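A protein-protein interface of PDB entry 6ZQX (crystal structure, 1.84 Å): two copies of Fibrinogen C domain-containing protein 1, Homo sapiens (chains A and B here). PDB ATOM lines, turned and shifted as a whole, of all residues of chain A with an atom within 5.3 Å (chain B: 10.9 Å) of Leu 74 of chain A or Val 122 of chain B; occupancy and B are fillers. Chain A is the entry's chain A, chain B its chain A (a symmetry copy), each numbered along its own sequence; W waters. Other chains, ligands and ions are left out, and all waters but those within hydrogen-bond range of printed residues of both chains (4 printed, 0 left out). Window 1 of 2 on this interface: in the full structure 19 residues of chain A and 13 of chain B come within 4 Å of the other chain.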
ATOM      1  N   VAL A  22      -8.553   9.608  13.023  1.00  0.00           N
ATOM      2  CA  VAL A  22      -8.799  10.466  14.212  1.00  0.00           C
ATOM      3  C   VAL A  22      -7.645  10.277  15.195  1.00  0.00           C
ATOM      4  O   VAL A  22      -7.293   9.122  15.489  1.00  0.00           O
ATOM      5  CB  VAL A  22     -10.163  10.143  14.833  1.00  0.00           C
ATOM      6  CG1 VAL A  22     -10.404  10.928  16.122  1.00  0.00           C
ATOM      7  CG2 VAL A  22     -11.265  10.413  13.833  1.00  0.00           C
ATOM      8  N   GLN A  35      -9.666  15.699  19.884  1.00  0.00           N
ATOM      9  CA  GLN A  35      -9.478  14.804  18.727  1.00  0.00           C
ATOM     10  C   GLN A  35      -9.735  15.593  17.448  1.00  0.00           C
ATOM     11  O   GLN A  35     -10.618  16.497  17.443  1.00  0.00           O
ATOM     12  CB  GLN A  35     -10.350  13.573  18.894  1.00  0.00           C
ATOM     13  CG  GLN A  35      -9.909  12.733  20.079  1.00  0.00           C
ATOM     14  CD  GLN A  35     -10.562  11.371  20.113  1.00  0.00           C
ATOM     15  OE1 GLN A  35     -11.738  11.216  19.810  1.00  0.00           O
ATOM     16  NE2 GLN A  35      -9.787  10.373  20.496  1.00  0.00           N
ATOM     17  N   VAL A  36      -9.023  15.206  16.389  1.00  0.00           N
ATOM     18  CA  VAL A  36      -9.124  15.815  15.034  1.00  0.00           C
ATOM     19  C   VAL A  36      -9.021  14.692  14.014  1.00  0.00           C
ATOM     20  O   VAL A  36      -8.517  13.588  14.377  1.00  0.00           O
ATOM     21  CB  VAL A  36      -8.022  16.860  14.805  1.00  0.00           C
ATOM     22  CG1 VAL A  36      -8.193  18.055  15.722  1.00  0.00           C
ATOM     23  CG2 VAL A  36      -6.620  16.267  14.960  1.00  0.00           C
ATOM     24  N   TYR A  37      -9.449  14.990  12.795  1.00  0.00           N
ATOM     25  CA  TYR A  37      -9.150  14.173  11.605  1.00  0.00           C
ATOM     26  C   TYR A  37      -7.834  14.659  10.997  1.00  0.00           C
ATOM     27  O   TYR A  37      -7.694  15.881  10.730  1.00  0.00           O
ATOM     28  CB  TYR A  37     -10.296  14.165  10.602  1.00  0.00           C
ATOM     29  CG  TYR A  37     -10.193  12.965   9.702  1.00  0.00           C
ATOM     30  CD1 TYR A  37      -9.347  12.967   8.600  1.00  0.00           C
ATOM     31  CD2 TYR A  37     -10.865  11.791  10.011  1.00  0.00           C
ATOM     32  CE1 TYR A  37      -9.226  11.844   7.792  1.00  0.00           C
ATOM     33  CE2 TYR A  37     -10.732  10.656   9.232  1.00  0.00           C
ATOM     34  CZ  TYR A  37      -9.907  10.685   8.119  1.00  0.00           C
ATOM     35  OH  TYR A  37      -9.800   9.555   7.350  1.00  0.00           O
ATOM     36  N   ARG A  52     -15.336  19.930   6.875  1.00  0.00           N
ATOM     37  CA  ARG A  52     -15.617  18.949   5.794  1.00  0.00           C
ATOM     38  C   ARG A  52     -17.102  18.992   5.440  1.00  0.00           C
ATOM     39  O   ARG A  52     -17.940  18.894   6.356  1.00  0.00           O
ATOM     40  CB  ARG A  52     -15.213  17.528   6.173  1.00  0.00           C
ATOM     41  CG  ARG A  52     -15.336  16.567   4.998  1.00  0.00           C
ATOM     42  CD  ARG A  52     -15.089  15.146   5.444  1.00  0.00           C
ATOM     43  NE  ARG A  52     -13.706  14.955   5.851  1.00  0.00           N
ATOM     44  CZ  ARG A  52     -13.299  14.436   7.013  1.00  0.00           C
ATOM     45  NH1 ARG A  52     -14.159  14.053   7.948  1.00  0.00           N
ATOM     46  NH2 ARG A  52     -12.010  14.263   7.223  1.00  0.00           N
ATOM     47  N   ASP A  69     -17.824  26.286  19.217  1.00  0.00           N
ATOM     48  CA  ASP A  69     -17.590  25.034  19.970  1.00  0.00           C
ATOM     49  C   ASP A  69     -17.419  23.833  19.034  1.00  0.00           C
ATOM     50  O   ASP A  69     -16.849  22.832  19.499  1.00  0.00           O
ATOM     51  CB  ASP A  69     -18.709  24.768  20.969  1.00  0.00           C
ATOM     52  CG  ASP A  69     -18.703  25.724  22.151  1.00  0.00           C
ATOM     53  OD1 ASP A  69     -17.639  26.277  22.460  1.00  0.00           O
ATOM     54  OD2 ASP A  69     -19.767  25.912  22.726  1.00  0.00           O
ATOM     55  N   GLY A  70     -17.892  23.916  17.786  1.00  0.00           N
ATOM     56  CA  GLY A  70     -17.794  22.808  16.817  1.00  0.00           C
ATOM     57  C   GLY A  70     -19.061  21.985  16.758  1.00  0.00           C
ATOM     58  O   GLY A  70     -19.876  22.008  17.728  1.00  0.00           O
ATOM     59  N   PHE A  71     -19.251  21.268  15.655  1.00  0.00           N
ATOM     60  CA  PHE A  71     -20.430  20.402  15.436  1.00  0.00           C
ATOM     61  C   PHE A  71     -20.103  19.359  14.369  1.00  0.00           C
ATOM     62  O   PHE A  71     -19.040  19.455  13.706  1.00  0.00           O
ATOM     63  CB  PHE A  71     -21.652  21.257  15.102  1.00  0.00           C
ATOM     64  CG  PHE A  71     -21.507  22.138  13.885  1.00  0.00           C
ATOM     65  CD1 PHE A  71     -21.793  21.642  12.627  1.00  0.00           C
ATOM     66  CD2 PHE A  71     -21.114  23.462  14.002  1.00  0.00           C
ATOM     67  CE1 PHE A  71     -21.657  22.439  11.503  1.00  0.00           C
ATOM     68  CE2 PHE A  71     -20.996  24.269  12.875  1.00  0.00           C
ATOM     69  CZ  PHE A  71     -21.284  23.761  11.634  1.00  0.00           C
ATOM     70  N   GLY A  72     -20.976  18.354  14.269  1.00  0.00           N
ATOM     71  CA  GLY A  72     -20.805  17.232  13.341  1.00  0.00           C
ATOM     72  C   GLY A  72     -19.833  16.207  13.885  1.00  0.00           C
ATOM     73  O   GLY A  72     -19.570  16.198  15.092  1.00  0.00           O
ATOM     74  N   ARG A  73     -19.341  15.331  13.028  1.00  0.00           N
ATOM     75  CA  ARG A  73     -18.497  14.186  13.448  1.00  0.00           C
ATOM     76  C   ARG A  73     -17.199  14.210  12.655  1.00  0.00           C
ATOM     77  O   ARG A  73     -17.231  14.544  11.435  1.00  0.00           O
ATOM     78  CB  ARG A  73     -19.274  12.879  13.319  1.00  0.00           C
ATOM     79  CG  ARG A  73     -20.461  12.861  14.267  1.00  0.00           C
ATOM     80  CD  ARG A  73     -21.248  11.582  14.251  1.00  0.00           C
ATOM     81  NE  ARG A  73     -22.392  11.724  15.142  1.00  0.00           N
ATOM     82  CZ  ARG A  73     -23.490  10.974  15.094  1.00  0.00           C
ATOM     83  NH1 ARG A  73     -23.599  10.005  14.201  1.00  0.00           N
ATOM     84  NH2 ARG A  73     -24.468  11.188  15.952  1.00  0.00           N
ATOM     85  N   LEU A  74     -16.120  13.826  13.326  1.00  0.00           N
ATOM     86  CA  LEU A  74     -14.750  13.918  12.758  1.00  0.00           C
ATOM     87  C   LEU A  74     -14.623  13.007  11.537  1.00  0.00           C
ATOM     88  O   LEU A  74     -13.834  13.353  10.652  1.00  0.00           O
ATOM     89  CB  LEU A  74     -13.729  13.548  13.832  1.00  0.00           C
ATOM     90  CG  LEU A  74     -13.644  14.528  14.996  1.00  0.00           C
ATOM     91  CD1 LEU A  74     -12.732  13.984  16.076  1.00  0.00           C
ATOM     92  CD2 LEU A  74     -13.153  15.889  14.537  1.00  0.00           C
ATOM     93  N   THR A  75     -15.384  11.917  11.503  1.00  0.00           N
ATOM     94  CA  THR A  75     -15.363  10.896  10.423  1.00  0.00           C
ATOM     95  C   THR A  75     -16.266  11.309   9.256  1.00  0.00           C
ATOM     96  O   THR A  75     -16.276  10.583   8.231  1.00  0.00           O
ATOM     97  CB  THR A  75     -15.807   9.535  10.959  1.00  0.00           C
ATOM     98  OG1 THR A  75     -17.024   9.745  11.672  1.00  0.00           O
ATOM     99  CG2 THR A  75     -14.759   8.903  11.844  1.00  0.00           C
ATOM    100  N   GLY A  76     -17.009  12.410   9.383  1.00  0.00           N
ATOM    101  CA  GLY A  76     -17.930  12.869   8.327  1.00  0.00           C
ATOM    102  C   GLY A  76     -17.892  14.382   8.175  1.00  0.00           C
ATOM    103  O   GLY A  76     -16.807  14.967   8.285  1.00  0.00           O
ATOM    104  N   HIS A  78     -18.228  18.081   9.343  1.00  0.00           N
ATOM    105  CA  HIS A  78     -18.020  18.717  10.664  1.00  0.00           C
ATOM    106  C   HIS A  78     -17.420  20.092  10.502  1.00  0.00           C
ATOM    107  O   HIS A  78     -16.909  20.434   9.431  1.00  0.00           O
ATOM    108  CB  HIS A  78     -17.157  17.851  11.585  1.00  0.00           C
ATOM    109  CG  HIS A  78     -15.725  17.686  11.174  1.00  0.00           C
ATOM    110  ND1 HIS A  78     -15.322  16.772  10.208  1.00  0.00           N
ATOM    111  CD2 HIS A  78     -14.600  18.266  11.638  1.00  0.00           C
ATOM    112  CE1 HIS A  78     -14.003  16.803  10.104  1.00  0.00           C
ATOM    113  NE2 HIS A  78     -13.535  17.715  10.971  1.00  0.00           N
ATOM    114  N   TRP A  79     -17.464  20.823  11.606  1.00  0.00           N
ATOM    115  CA  TRP A  79     -16.738  22.090  11.812  1.00  0.00           C
ATOM    116  C   TRP A  79     -16.056  21.949  13.167  1.00  0.00           C
ATOM    117  O   TRP A  79     -16.768  21.655  14.135  1.00  0.00           O
ATOM    118  CB  TRP A  79     -17.708  23.271  11.780  1.00  0.00           C
ATOM    119  CG  TRP A  79     -17.061  24.570  12.146  1.00  0.00           C
ATOM    120  CD1 TRP A  79     -17.097  25.208  13.352  1.00  0.00           C
ATOM    121  CD2 TRP A  79     -16.295  25.404  11.274  1.00  0.00           C
ATOM    122  NE1 TRP A  79     -16.408  26.385  13.299  1.00  0.00           N
ATOM    123  CE2 TRP A  79     -15.920  26.541  12.022  1.00  0.00           C
ATOM    124  CE3 TRP A  79     -15.920  25.317   9.929  1.00  0.00           C
ATOM    125  CZ2 TRP A  79     -15.175  27.570  11.457  1.00  0.00           C
ATOM    126  CZ3 TRP A  79     -15.193  26.344   9.372  1.00  0.00           C
ATOM    127  CH2 TRP A  79     -14.801  27.441  10.138  1.00  0.00           C
ATOM    128  N   LEU A  80     -14.730  22.053  13.214  1.00  0.00           N
ATOM    129  CA  LEU A  80     -13.963  21.689  14.434  1.00  0.00           C
ATOM    130  C   LEU A  80     -14.252  22.705  15.545  1.00  0.00           C
ATOM    131  O   LEU A  80     -14.092  22.349  16.726  1.00  0.00           O
ATOM    132  CB  LEU A  80     -12.476  21.655  14.094  1.00  0.00           C
ATOM    133  CG  LEU A  80     -11.543  21.211  15.214  1.00  0.00           C
ATOM    134  CD1 LEU A  80     -11.840  19.779  15.628  1.00  0.00           C
ATOM    135  CD2 LEU A  80     -10.105  21.342  14.758  1.00  0.00           C
ATOM    136  N   GLY A  81     -14.622  23.934  15.186  1.00  0.00           N
ATOM    137  CA  GLY A  81     -14.890  24.986  16.181  1.00  0.00           C
ATOM    138  C   GLY A  81     -13.804  26.048  16.215  1.00  0.00           C
ATOM    139  O   GLY A  81     -12.615  25.714  16.271  1.00  0.00           O
ATOM    140  N   ARG A  84     -11.048  25.919  18.793  1.00  0.00           N
ATOM    141  CA  ARG A  84      -9.990  24.923  18.485  1.00  0.00           C
ATOM    142  C   ARG A  84      -9.111  25.447  17.354  1.00  0.00           C
ATOM    143  O   ARG A  84      -7.895  25.297  17.450  1.00  0.00           O
ATOM    144  CB  ARG A  84     -10.597  23.570  18.135  1.00  0.00           C
ATOM    145  CG  ARG A  84     -11.376  22.982  19.298  1.00  0.00           C
ATOM    146  CD  ARG A  84     -11.782  21.557  19.070  1.00  0.00           C
ATOM    147  NE  ARG A  84     -12.463  21.051  20.257  1.00  0.00           N
ATOM    148  CZ  ARG A  84     -13.759  21.056  20.448  1.00  0.00           C
ATOM    149  NH1 ARG A  84     -14.583  21.518  19.522  1.00  0.00           N
ATOM    150  NH2 ARG A  84     -14.238  20.586  21.583  1.00  0.00           N
ATOM    151  N   HIS B  29      -8.161  13.459  27.778  1.00  0.00           N
ATOM    152  CA  HIS B  29      -8.706  14.817  27.522  1.00  0.00           C
ATOM    153  C   HIS B  29      -9.498  15.343  28.725  1.00  0.00           C
ATOM    154  O   HIS B  29     -10.274  16.283  28.545  1.00  0.00           O
ATOM    155  CB  HIS B  29      -9.519  14.789  26.237  1.00  0.00           C
ATOM    156  CG  HIS B  29      -8.693  14.450  25.054  1.00  0.00           C
ATOM    157  ND1 HIS B  29      -7.604  15.211  24.692  1.00  0.00           N
ATOM    158  CD2 HIS B  29      -8.804  13.454  24.142  1.00  0.00           C
ATOM    159  CE1 HIS B  29      -7.082  14.708  23.582  1.00  0.00           C
ATOM    160  NE2 HIS B  29      -7.798  13.626  23.223  1.00  0.00           N
ATOM    161  N   HIS B  86     -17.767   9.856  28.170  1.00  0.00           N
ATOM    162  CA  HIS B  86     -17.149  10.268  26.885  1.00  0.00           C
ATOM    163  C   HIS B  86     -15.619  10.299  27.042  1.00  0.00           C
ATOM    164  O   HIS B  86     -14.936   9.695  26.211  1.00  0.00           O
ATOM    165  CB  HIS B  86     -17.735  11.595  26.405  1.00  0.00           C
ATOM    166  CG  HIS B  86     -17.024  12.118  25.204  1.00  0.00           C
ATOM    167  ND1 HIS B  86     -15.988  13.041  25.296  1.00  0.00           N
ATOM    168  CD2 HIS B  86     -17.137  11.799  23.894  1.00  0.00           C
ATOM    169  CE1 HIS B  86     -15.499  13.270  24.088  1.00  0.00           C
ATOM    170  NE2 HIS B  86     -16.197  12.535  23.213  1.00  0.00           N
ATOM    171  N   THR B  90     -13.415   7.439  24.730  1.00  0.00           N
ATOM    172  CA  THR B  90     -12.703   7.959  23.532  1.00  0.00           C
ATOM    173  C   THR B  90     -11.184   7.785  23.640  1.00  0.00           C
ATOM    174  O   THR B  90     -10.512   8.084  22.646  1.00  0.00           O
ATOM    175  CB  THR B  90     -13.037   9.431  23.248  1.00  0.00           C
ATOM    176  OG1 THR B  90     -12.784  10.247  24.390  1.00  0.00           O
ATOM    177  CG2 THR B  90     -14.473   9.618  22.831  1.00  0.00           C
ATOM    178  N   VAL B 117     -19.386   6.390  23.873  1.00  0.00           N
ATOM    179  CA  VAL B 117     -20.390   7.476  23.918  1.00  0.00           C
ATOM    180  C   VAL B 117     -19.743   8.685  23.232  1.00  0.00           C
ATOM    181  O   VAL B 117     -18.650   9.096  23.663  1.00  0.00           O
ATOM    182  CB  VAL B 117     -20.806   7.694  25.383  1.00  0.00           C
ATOM    183  CG1 VAL B 117     -21.499   8.997  25.634  1.00  0.00           C
ATOM    184  CG2 VAL B 117     -21.659   6.532  25.875  1.00  0.00           C
ATOM    185  N   GLY B 118     -20.375   9.176  22.167  1.00  0.00           N
ATOM    186  CA  GLY B 118     -19.935  10.371  21.422  1.00  0.00           C
ATOM    187  C   GLY B 118     -18.558  10.192  20.789  1.00  0.00           C
ATOM    188  O   GLY B 118     -17.821  11.175  20.736  1.00  0.00           O
ATOM    189  N   LEU B 119     -18.224   8.996  20.289  1.00  0.00           N
ATOM    190  CA  LEU B 119     -16.822   8.604  19.962  1.00  0.00           C
ATOM    191  C   LEU B 119     -16.157   9.574  18.962  1.00  0.00           C
ATOM    192  O   LEU B 119     -14.924   9.817  19.095  1.00  0.00           O
ATOM    193  CB  LEU B 119     -16.776   7.162  19.437  1.00  0.00           C
ATOM    194  CG  LEU B 119     -16.855   6.052  20.497  1.00  0.00           C
ATOM    195  CD1 LEU B 119     -16.448   4.720  19.898  1.00  0.00           C
ATOM    196  CD2 LEU B 119     -15.991   6.347  21.716  1.00  0.00           C
ATOM    197  N   PHE B 120     -16.882  10.052  17.966  1.00  0.00           N
ATOM    198  CA  PHE B 120     -16.315  10.911  16.887  1.00  0.00           C
ATOM    199  C   PHE B 120     -16.992  12.285  16.857  1.00  0.00           C
ATOM    200  O   PHE B 120     -16.773  13.057  15.920  1.00  0.00           O
ATOM    201  CB  PHE B 120     -16.446  10.175  15.550  1.00  0.00           C
ATOM    202  CG  PHE B 120     -15.659   8.888  15.520  1.00  0.00           C
ATOM    203  CD1 PHE B 120     -14.273   8.912  15.578  1.00  0.00           C
ATOM    204  CD2 PHE B 120     -16.293   7.657  15.524  1.00  0.00           C
ATOM    205  CE1 PHE B 120     -13.536   7.735  15.577  1.00  0.00           C
ATOM    206  CE2 PHE B 120     -15.555   6.482  15.535  1.00  0.00           C
ATOM    207  CZ  PHE B 120     -14.181   6.521  15.549  1.00  0.00           C
ATOM    208  N   SER B 121     -17.791  12.600  17.867  1.00  0.00           N
ATOM    209  CA  SER B 121     -18.564  13.864  17.970  1.00  0.00           C
ATOM    210  C   SER B 121     -17.601  15.023  18.257  1.00  0.00           C
ATOM    211  O   SER B 121     -16.877  14.952  19.258  1.00  0.00           O
ATOM    212  CB  SER B 121     -19.598  13.766  19.046  1.00  0.00           C
ATOM    213  OG  SER B 121     -20.452  12.651  18.830  1.00  0.00           O
ATOM    214  N   VAL B 122     -17.614  16.080  17.453  1.00  0.00           N
ATOM    215  CA  VAL B 122     -16.787  17.289  17.737  1.00  0.00           C
ATOM    216  C   VAL B 122     -17.235  17.908  19.063  1.00  0.00           C
ATOM    217  O   VAL B 122     -16.379  18.215  19.878  1.00  0.00           O
ATOM    218  CB  VAL B 122     -16.873  18.310  16.594  1.00  0.00           C
ATOM    219  CG1 VAL B 122     -16.145  19.593  16.957  1.00  0.00           C
ATOM    220  CG2 VAL B 122     -16.354  17.708  15.309  1.00  0.00           C
ATOM    221  N   ASP B 123     -18.540  18.051  19.268  1.00  0.00           N
ATOM    222  CA  ASP B 123     -19.145  18.493  20.546  1.00  0.00           C
ATOM    223  C   ASP B 123     -20.056  17.360  20.998  1.00  0.00           C
ATOM    224  O   ASP B 123     -21.204  17.286  20.586  1.00  0.00           O
ATOM    225  CB  ASP B 123     -19.847  19.838  20.366  1.00  0.00           C
ATOM    226  CG  ASP B 123     -20.533  20.379  21.619  1.00  0.00           C
ATOM    227  OD1 ASP B 123     -20.642  19.635  22.596  1.00  0.00           O
ATOM    228  OD2 ASP B 123     -20.986  21.538  21.578  1.00  0.00           O
ATOM    229  N   PRO B 124     -19.552  16.401  21.796  1.00  0.00           N
ATOM    230  CA  PRO B 124     -20.374  15.254  22.204  1.00  0.00           C
ATOM    231  C   PRO B 124     -21.671  15.670  22.910  1.00  0.00           C
ATOM    232  O   PRO B 124     -22.673  14.961  22.790  1.00  0.00           O
ATOM    233  CB  PRO B 124     -19.457  14.406  23.101  1.00  0.00           C
ATOM    234  CG  PRO B 124     -18.308  15.344  23.472  1.00  0.00           C
ATOM    235  CD  PRO B 124     -18.186  16.348  22.341  1.00  0.00           C
ATOM    236  N   GLU B 125     -21.660  16.785  23.643  1.00  0.00           N
ATOM    237  CA  GLU B 125     -22.900  17.246  24.308  1.00  0.00           C
ATOM    238  C   GLU B 125     -23.928  17.677  23.246  1.00  0.00           C
ATOM    239  O   GLU B 125     -25.079  17.207  23.331  1.00  0.00           O
ATOM    240  CB  GLU B 125     -22.646  18.351  25.331  1.00  0.00           C
ATOM    241  CG  GLU B 125     -23.935  18.725  26.037  1.00  0.00           C
ATOM    242  CD  GLU B 125     -23.889  19.898  26.990  1.00  0.00           C
ATOM    243  OE1 GLU B 125     -22.835  20.539  27.072  1.00  0.00           O
ATOM    244  OE2 GLU B 125     -24.908  20.146  27.650  1.00  0.00           O
ATOM    245  N   GLU B 126     -23.554  18.542  22.292  1.00  0.00           N
ATOM    246  CA  GLU B 126     -24.498  19.036  21.248  1.00  0.00           C
ATOM    247  C   GLU B 126     -24.990  17.840  20.430  1.00  0.00           C
ATOM    248  O   GLU B 126     -26.206  17.795  20.132  1.00  0.00           O
ATOM    249  CB  GLU B 126     -23.903  20.138  20.357  1.00  0.00           C
ATOM    250  CG  GLU B 126     -23.031  19.661  19.189  1.00  0.00           C
ATOM    251  CD  GLU B 126     -23.687  19.448  17.828  1.00  0.00           C
ATOM    252  OE1 GLU B 126     -24.646  20.178  17.510  1.00  0.00           O
ATOM    253  OE2 GLU B 126     -23.225  18.568  17.075  1.00  0.00           O
ATOM    254  N   ASP B 127     -24.108  16.876  20.161  1.00  0.00           N
ATOM    255  CA  ASP B 127     -24.390  15.683  19.312  1.00  0.00           C
ATOM    256  C   ASP B 127     -25.206  14.639  20.094  1.00  0.00           C
ATOM    257  O   ASP B 127     -25.547  13.615  19.498  1.00  0.00           O
ATOM    258  CB  ASP B 127     -23.082  15.074  18.804  1.00  0.00           C
ATOM    259  CG  ASP B 127     -23.220  14.216  17.558  1.00  0.00           C
ATOM    260  OD1 ASP B 127     -24.165  14.460  16.786  1.00  0.00           O
ATOM    261  OD2 ASP B 127     -22.387  13.305  17.380  1.00  0.00           O
ATOM    262  N   GLY B 128     -25.425  14.832  21.399  1.00  0.00           N
ATOM    263  CA  GLY B 128     -26.306  13.966  22.214  1.00  0.00           C
ATOM    264  C   GLY B 128     -25.638  12.666  22.632  1.00  0.00           C
ATOM    265  O   GLY B 128     -26.369  11.659  22.851  1.00  0.00           O
ATOM    266  N   TYR B 129     -24.311  12.672  22.807  1.00  0.00           N
ATOM    267  CA  TYR B 129     -23.533  11.541  23.382  1.00  0.00           C
ATOM    268  C   TYR B 129     -23.990  10.216  22.776  1.00  0.00           C
ATOM    269  O   TYR B 129     -24.377   9.283  23.488  1.00  0.00           O
ATOM    270  CB  TYR B 129     -23.725  11.526  24.902  1.00  0.00           C
ATOM    271  CG  TYR B 129     -23.107  12.697  25.624  1.00  0.00           C
ATOM    272  CD1 TYR B 129     -21.732  12.839  25.712  1.00  0.00           C
ATOM    273  CD2 TYR B 129     -23.898  13.656  26.229  1.00  0.00           C
ATOM    274  CE1 TYR B 129     -21.160  13.909  26.380  1.00  0.00           C
ATOM    275  CE2 TYR B 129     -23.348  14.724  26.914  1.00  0.00           C
ATOM    276  CZ  TYR B 129     -21.974  14.852  26.980  1.00  0.00           C
ATOM    277  OH  TYR B 129     -21.444  15.909  27.644  1.00  0.00           O
ATOM    278  N   PRO B 130     -24.000  10.083  21.436  1.00  0.00           N
ATOM    279  CA  PRO B 130     -24.519   8.883  20.791  1.00  0.00           C
ATOM    280  C   PRO B 130     -23.771   7.593  21.148  1.00  0.00           C
ATOM    281  O   PRO B 130     -22.571   7.597  21.341  1.00  0.00           O
ATOM    282  CB  PRO B 130     -24.351   9.186  19.300  1.00  0.00           C
ATOM    283  CG  PRO B 130     -23.248  10.211  19.275  1.00  0.00           C
ATOM    284  CD  PRO B 130     -23.575  11.094  20.453  1.00  0.00           C
ATOM    285  N   ARG B 151     -28.844   8.759  20.079  1.00  0.00           N
ATOM    286  CA  ARG B 151     -28.425   9.837  21.002  1.00  0.00           C
ATOM    287  C   ARG B 151     -29.068   9.582  22.363  1.00  0.00           C
ATOM    288  O   ARG B 151     -30.013   8.776  22.468  1.00  0.00           O
ATOM    289  CB  ARG B 151     -28.804  11.193  20.412  1.00  0.00           C
ATOM    290  CG  ARG B 151     -28.040  11.520  19.137  1.00  0.00           C
ATOM    291  CD  ARG B 151     -28.494  12.850  18.563  1.00  0.00           C
ATOM    292  NE  ARG B 151     -27.532  13.416  17.616  1.00  0.00           N
ATOM    293  CZ  ARG B 151     -27.562  13.247  16.300  1.00  0.00           C
ATOM    294  NH1 ARG B 151     -28.508  12.509  15.740  1.00  0.00           N
ATOM    295  NH2 ARG B 151     -26.641  13.818  15.538  1.00  0.00           N
HETATM  296  O   HOH W   1     -20.606  17.252  17.519  1.00  0.00           O
HETATM  297  O   HOH W   2     -12.607   8.421  19.358  1.00  0.00           O
HETATM  298  O   HOH W   3     -21.730  23.028  19.449  1.00  0.00           O
HETATM  299  O   HOH W   4     -24.141  18.634  14.200  1.00  0.00           O
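The backbone carbonyl oxygen (O) of Leu 74 of chain A is in hydrogen-bond range of the guanidinium group (NH1) of Arg 52 of chain A (2.8 Å). O of Arg 73 of chain A lies within hydrogen-bond range of ND1 of His 78 of chain A, at 3.2 Å. NH1 of Arg 84 of chain A sits at hydrogen-bond distance from O of Leu 80 of chain A (3.0 Å). The backbone NH (N) of Glu 126 of chain B lies within hydrogen-bond range of the side-chain carboxylate (OD1) of Asp 123 of chain B, at 3.1 Å.
Water W3 lies within hydrogen-bond range of OD2 of Asp 123 of chain B (2.7 Å) and O of Gly 70 of chain A (2.7 Å). Water W2 lies within hydrogen-bond range of the backbone carbonyl oxygen of Leu 119 of chain B (2.7 Å) and the side-chain amide oxygen of Gln 35 of chain A (3.0 Å). Water W1 lies within hydrogen-bond range of N of Asp 123 of chain B (2.8 Å), O of Gly 72 of chain A (2.8 Å), OE2 of Glu 126 of chain B (3.0 Å) and N of Val 122 of chain B (3.2 Å).
Of the 18 printed residues of chain A, 13 touch a printed residue of chain B. Printed residues of chain A that touch a printed residue of chain B: Val 22, Gln 35, Asp 69, Gly 70, Phe 71, Gly 72, Arg 73, Leu 74, Thr 75, His 78, Trp 79, Leu 80 and Arg 84. Of the 18 printed residues of chain B, 11 touch a printed residue of chain A. Printed residues of chain B that touch a printed residue of chain A: His 29, Thr 90, Leu 119, Phe 120, Ser 121, Val 122, Asp 123, Glu 126, Asp 127, Pro 130 and Arg 151. Hydrophobic or aromatic side chains of chain B that line the printed part of chain A: His 29, Phe 120, Val 122 and Pro 130.
The backbone carbonyl oxygen (O) of Thr 90 of chain B is in hydrogen-bond range of the side-chain amide nitrogen (NE2) of Gln 35 of chain A (3.2 Å). The backbone NH of Val 122 of chain B is in hydrogen-bond range of the backbone carbonyl oxygen of Gly 72 of chain A (3.1 Å). The guanidinium group (NE) of Arg 73 of chain A is in salt-bridge range of the side-chain carboxylate (OD2) of Asp 127 of chain B (2.7 Å). The backbone NH of Leu 74 of chain A is in hydrogen-bond range of the backbone carbonyl oxygen of Phe 120 of chain B, 2.8 Å away. NH2 of Arg 151 of chain B sits close to NH2 of Arg 73 of chain A (3.4 Å).
Gln 35 of chain A touches three residues of chain B. No residue of chain B comes within 4 Å of Val 36 of chain A. No residue of chain B comes within 4 Å of Tyr 37 of chain A. Arg 52 of chain A touches none of the printed residues of chain B. Gly 72 of chain A touches just these residues of chain B: Ser 121 (3.8 Å), Val 122 (3.1 Å) and Glu 126 (3.6 Å). Of the printed residues of chain B, Arg 73 of chain A touches Phe 120 (3.2 Å), Asp 127 (2.7 Å), Pro 130 (3.7 Å) and Arg 151 (3.4 Å). Leu 74 of chain A touches two residues of chain B. Of chain B, only Phe 120 comes within 4 Å of Thr 75 of chain A. Of chain B, only Val 122 (3.8 Å) comes within 4 Å of His 78 of chain A. Gly 118 of chain B touches none of the printed residues of chain A. Of the printed residues of chain A, Leu 119 of chain B touches Gln 35 (3.6 Å). Val 122 of chain B touches eight residues of chain A. The nearest residue of chain B that does not touch Leu 74 of chain A is Ser 121 of chain B (5.0 Å).
His 29 of chain B touches Gln 35 of chain A. Val 122 of chain B touches Phe 71 of chain A (CG2 to O, 3.6 Å). Phe 71 of chain A touches Glu 126 of chain B. Ser 121 of chain B touches Gly 72 of chain A. Arg 73 of chain A touches Phe 120 of chain B (CA to O, 3.2 Å). CG of Pro 130 of chain B touches NH2 of Arg 73 of chain A, 3.7 Å away. Thr 75 of chain A touches Phe 120 of chain B (CG2 to CD1, 3.8 Å). O of Trp 79 of chain A touches CG1 of Val 122 of chain B, 3.6 Å away. Val 122 of chain B touches Leu 80 of chain A (CG1 to O, 3.4 Å).
No position is printed for both chains.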
